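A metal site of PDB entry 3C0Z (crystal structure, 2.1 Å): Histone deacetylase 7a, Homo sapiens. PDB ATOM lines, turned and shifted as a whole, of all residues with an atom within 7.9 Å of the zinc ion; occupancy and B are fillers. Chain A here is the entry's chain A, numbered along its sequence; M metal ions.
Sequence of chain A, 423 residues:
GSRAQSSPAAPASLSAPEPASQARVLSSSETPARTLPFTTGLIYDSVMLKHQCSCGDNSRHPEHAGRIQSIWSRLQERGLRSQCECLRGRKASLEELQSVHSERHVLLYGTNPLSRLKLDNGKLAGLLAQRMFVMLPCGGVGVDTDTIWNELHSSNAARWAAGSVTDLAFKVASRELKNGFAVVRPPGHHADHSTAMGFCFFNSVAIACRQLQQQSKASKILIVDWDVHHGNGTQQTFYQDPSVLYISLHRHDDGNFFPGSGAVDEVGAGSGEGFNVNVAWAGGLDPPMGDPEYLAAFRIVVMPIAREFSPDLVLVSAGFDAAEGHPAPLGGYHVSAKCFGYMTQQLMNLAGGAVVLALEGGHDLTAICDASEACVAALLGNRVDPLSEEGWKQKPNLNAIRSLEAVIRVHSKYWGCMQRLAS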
ATOM      1  N   GLN A  52       2.836  21.537 -21.356  1.00  0.00           N
ATOM      2  CA  GLN A  52       1.549  21.874 -20.760  1.00  0.00           C
ATOM      3  C   GLN A  52       1.142  20.759 -19.824  1.00  0.00           C
ATOM      4  O   GLN A  52       1.385  19.578 -20.118  1.00  0.00           O
ATOM      5  CB  GLN A  52       0.415  22.056 -21.825  1.00  0.00           C
ATOM      6  CG  GLN A  52       0.824  22.692 -23.144  1.00  0.00           C
ATOM      7  CD  GLN A  52      -0.276  22.696 -24.213  1.00  0.00           C
ATOM      8  OE1 GLN A  52      -0.135  23.352 -25.258  1.00  0.00           O
ATOM      9  NE2 GLN A  52      -1.371  21.958 -23.965  1.00  0.00           N
ATOM     10  N   CYS A  53       0.523  21.105 -18.703  1.00  0.00           N
ATOM     11  CA  CYS A  53       0.021  20.041 -17.828  1.00  0.00           C
ATOM     12  C   CYS A  53      -1.013  19.147 -18.581  1.00  0.00           C
ATOM     13  O   CYS A  53      -1.724  19.601 -19.508  1.00  0.00           O
ATOM     14  CB  CYS A  53      -0.585  20.605 -16.534  1.00  0.00           C
ATOM     15  SG  CYS A  53      -0.958  19.287 -15.354  1.00  0.00           S
ATOM     16  N   SER A  54      -1.079  17.880 -18.192  1.00  0.00           N
ATOM     17  CA  SER A  54      -2.086  16.991 -18.762  1.00  0.00           C
ATOM     18  C   SER A  54      -3.538  17.318 -18.347  1.00  0.00           C
ATOM     19  O   SER A  54      -4.469  16.920 -19.030  1.00  0.00           O
ATOM     20  CB  SER A  54      -1.732  15.530 -18.489  1.00  0.00           C
ATOM     21  OG  SER A  54      -1.460  15.366 -17.125  1.00  0.00           O
ATOM     22  N   CYS A  55      -3.707  18.074 -17.248  1.00  0.00           N
ATOM     23  CA  CYS A  55      -5.040  18.513 -16.756  1.00  0.00           C
ATOM     24  C   CYS A  55      -5.709  19.491 -17.703  1.00  0.00           C
ATOM     25  O   CYS A  55      -6.899  19.777 -17.555  1.00  0.00           O
ATOM     26  CB  CYS A  55      -4.930  19.165 -15.382  1.00  0.00           C
ATOM     27  SG  CYS A  55      -4.438  20.916 -15.438  1.00  0.00           S
ATOM     28  N   GLY A  56      -4.951  20.024 -18.662  1.00  0.00           N
ATOM     29  CA  GLY A  56      -5.497  20.873 -19.734  1.00  0.00           C
ATOM     30  C   GLY A  56      -6.145  22.178 -19.289  1.00  0.00           C
ATOM     31  O   GLY A  56      -7.088  22.641 -19.921  1.00  0.00           O
ATOM     32  N   ASP A  57      -5.646  22.778 -18.212  1.00  0.00           N
ATOM     33  CA  ASP A  57      -6.237  23.996 -17.636  1.00  0.00           C
ATOM     34  C   ASP A  57      -5.171  25.063 -17.347  1.00  0.00           C
ATOM     35  O   ASP A  57      -4.451  24.976 -16.343  1.00  0.00           O
ATOM     36  CB  ASP A  57      -6.971  23.638 -16.334  1.00  0.00           C
ATOM     37  CG  ASP A  57      -7.867  24.783 -15.809  1.00  0.00           C
ATOM     38  OD1 ASP A  57      -8.140  25.761 -16.565  1.00  0.00           O
ATOM     39  OD2 ASP A  57      -8.264  24.669 -14.629  1.00  0.00           O
ATOM     40  N   ASN A  58      -5.083  26.054 -18.237  1.00  0.00           N
ATOM     41  CA  ASN A  58      -4.207  27.212 -18.077  1.00  0.00           C
ATOM     42  C   ASN A  58      -4.491  28.055 -16.812  1.00  0.00           C
ATOM     43  O   ASN A  58      -3.652  28.852 -16.397  1.00  0.00           O
ATOM     44  CB  ASN A  58      -4.249  28.087 -19.327  1.00  0.00           C
ATOM     45  CG  ASN A  58      -3.524  27.467 -20.498  1.00  0.00           C
ATOM     46  OD1 ASN A  58      -2.924  26.395 -20.358  1.00  0.00           O
ATOM     47  ND2 ASN A  58      -3.536  28.141 -21.660  1.00  0.00           N
ATOM     48  N   ARG A  60      -4.942  26.934 -13.548  1.00  0.00           N
ATOM     49  CA  ARG A  60      -4.137  26.621 -12.345  1.00  0.00           C
ATOM     50  C   ARG A  60      -2.610  26.592 -12.593  1.00  0.00           C
ATOM     51  O   ARG A  60      -1.837  26.157 -11.738  1.00  0.00           O
ATOM     52  CB  ARG A  60      -4.625  25.368 -11.580  1.00  0.00           C
ATOM     53  CG  ARG A  60      -4.957  24.152 -12.422  1.00  0.00           C
ATOM     54  CD  ARG A  60      -5.886  23.229 -11.629  1.00  0.00           C
ATOM     55  NE  ARG A  60      -6.637  22.291 -12.466  1.00  0.00           N
ATOM     56  CZ  ARG A  60      -7.629  21.520 -12.036  1.00  0.00           C
ATOM     57  NH1 ARG A  60      -8.023  21.559 -10.769  1.00  0.00           N
ATOM     58  NH2 ARG A  60      -8.239  20.692 -12.874  1.00  0.00           N
ATOM     59  N   HIS A  61      -2.212  27.078 -13.774  1.00  0.00           N
ATOM     60  CA  HIS A  61      -0.848  26.930 -14.283  1.00  0.00           C
ATOM     61  C   HIS A  61      -0.460  28.188 -15.060  1.00  0.00           C
ATOM     62  O   HIS A  61      -0.570  28.220 -16.295  1.00  0.00           O
ATOM     63  CB  HIS A  61      -0.743  25.699 -15.197  1.00  0.00           C
ATOM     64  CG  HIS A  61      -1.120  24.398 -14.541  1.00  0.00           C
ATOM     65  ND1 HIS A  61      -0.561  23.972 -13.349  1.00  0.00           N
ATOM     66  CD2 HIS A  61      -1.960  23.409 -14.939  1.00  0.00           C
ATOM     67  CE1 HIS A  61      -1.052  22.784 -13.035  1.00  0.00           C
ATOM     68  NE2 HIS A  61      -1.908  22.421 -13.981  1.00  0.00           N
ATOM     69  N   LEU A 136       0.191  16.088  -8.726  1.00  0.00           N
ATOM     70  CA  LEU A 136      -0.334  17.396  -8.460  1.00  0.00           C
ATOM     71  C   LEU A 136      -1.826  17.258  -8.152  1.00  0.00           C
ATOM     72  O   LEU A 136      -2.446  16.255  -8.561  1.00  0.00           O
ATOM     73  CB  LEU A 136      -0.099  18.327  -9.658  1.00  0.00           C
ATOM     74  CG  LEU A 136       1.369  18.446 -10.072  1.00  0.00           C
ATOM     75  CD1 LEU A 136       1.511  19.354 -11.304  1.00  0.00           C
ATOM     76  CD2 LEU A 136       2.224  18.952  -8.940  1.00  0.00           C
ATOM     77  N   PRO A 137      -2.389  18.216  -7.389  1.00  0.00           N
ATOM     78  CA  PRO A 137      -3.832  18.346  -7.126  1.00  0.00           C
ATOM     79  C   PRO A 137      -4.651  18.104  -8.381  1.00  0.00           C
ATOM     80  O   PRO A 137      -5.669  17.424  -8.296  1.00  0.00           O
ATOM     81  CB  PRO A 137      -3.993  19.796  -6.674  1.00  0.00           C
ATOM     82  CG  PRO A 137      -2.635  20.174  -6.042  1.00  0.00           C
ATOM     83  CD  PRO A 137      -1.585  19.252  -6.671  1.00  0.00           C
ATOM     84  N   CYS A 138      -4.201  18.616  -9.534  1.00  0.00           N
ATOM     85  CA  CYS A 138      -4.955  18.523 -10.802  1.00  0.00           C
ATOM     86  C   CYS A 138      -4.858  17.141 -11.478  1.00  0.00           C
ATOM     87  O   CYS A 138      -5.426  16.923 -12.547  1.00  0.00           O
ATOM     88  CB  CYS A 138      -4.420  19.601 -11.755  1.00  0.00           C
ATOM     89  SG  CYS A 138      -2.660  19.334 -12.302  1.00  0.00           S
ATOM     90  N   GLY A 139      -4.127  16.219 -10.843  1.00  0.00           N
ATOM     91  CA  GLY A 139      -3.821  14.890 -11.424  1.00  0.00           C
ATOM     92  C   GLY A 139      -2.645  14.762 -12.410  1.00  0.00           C
ATOM     93  O   GLY A 139      -2.185  13.641 -12.714  1.00  0.00           O
ATOM     94  N   GLY A 140      -2.126  15.884 -12.888  1.00  0.00           N
ATOM     95  CA  GLY A 140      -0.928  15.872 -13.710  1.00  0.00           C
ATOM     96  C   GLY A 140       0.321  15.530 -12.911  1.00  0.00           C
ATOM     97  O   GLY A 140       0.325  15.569 -11.673  1.00  0.00           O
ATOM     98  N   VAL A 141       1.387  15.209 -13.623  1.00  0.00           N
ATOM     99  CA  VAL A 141       2.671  14.929 -12.994  1.00  0.00           C
ATOM    100  C   VAL A 141       3.393  16.261 -12.814  1.00  0.00           C
ATOM    101  O   VAL A 141       3.265  17.155 -13.645  1.00  0.00           O
ATOM    102  CB  VAL A 141       3.514  13.988 -13.875  1.00  0.00           C
ATOM    103  CG1 VAL A 141       4.976  13.770 -13.291  1.00  0.00           C
ATOM    104  CG2 VAL A 141       2.816  12.700 -13.976  1.00  0.00           C
ATOM    105  N   THR A 145       4.711  21.443  -6.708  1.00  0.00           N
ATOM    106  CA  THR A 145       3.329  21.978  -6.871  1.00  0.00           C
ATOM    107  C   THR A 145       3.120  22.820  -8.126  1.00  0.00           C
ATOM    108  O   THR A 145       2.135  22.661  -8.853  1.00  0.00           O
ATOM    109  CB  THR A 145       2.848  22.807  -5.603  1.00  0.00           C
ATOM    110  OG1 THR A 145       3.667  23.992  -5.421  1.00  0.00           O
ATOM    111  CG2 THR A 145       2.913  21.965  -4.324  1.00  0.00           C
ATOM    112  N   ILE A 148       5.210  21.890 -13.514  1.00  0.00           N
ATOM    113  CA  ILE A 148       4.515  20.770 -14.143  1.00  0.00           C
ATOM    114  C   ILE A 148       5.467  20.021 -15.065  1.00  0.00           C
ATOM    115  O   ILE A 148       6.477  20.577 -15.506  1.00  0.00           O
ATOM    116  CB  ILE A 148       3.252  21.217 -14.897  1.00  0.00           C
ATOM    117  CG1 ILE A 148       3.601  21.856 -16.251  1.00  0.00           C
ATOM    118  CG2 ILE A 148       2.398  22.116 -14.003  1.00  0.00           C
ATOM    119  CD1 ILE A 148       3.741  20.869 -17.473  1.00  0.00           C
HETATM  120 ZN    ZN M   1      -2.585  20.566 -14.142  1.00  0.00          ZN
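The backbone NH (N) of Asp 57 lies close to the side-chain sulfur (SG) of Cys 55 (3.6 Å).
The backbone NH (N) of Gly 140 lies close to the side-chain sulfur (SG) of Cys 138, at 3.5 Å.
Four residues have an atom within 4 Å of the zinc ion: Cys 53, Cys 55, His 61 and Cys 138.
The zinc ion is bound by a ring nitrogen (NE2) of His 61 (2.0 Å), the side-chain sulfur of Cys 138 (2.2 Å), the side-chain sulfur of Cys 55 (2.3 Å) and the side-chain sulfur of Cys 53 (2.4 Å).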
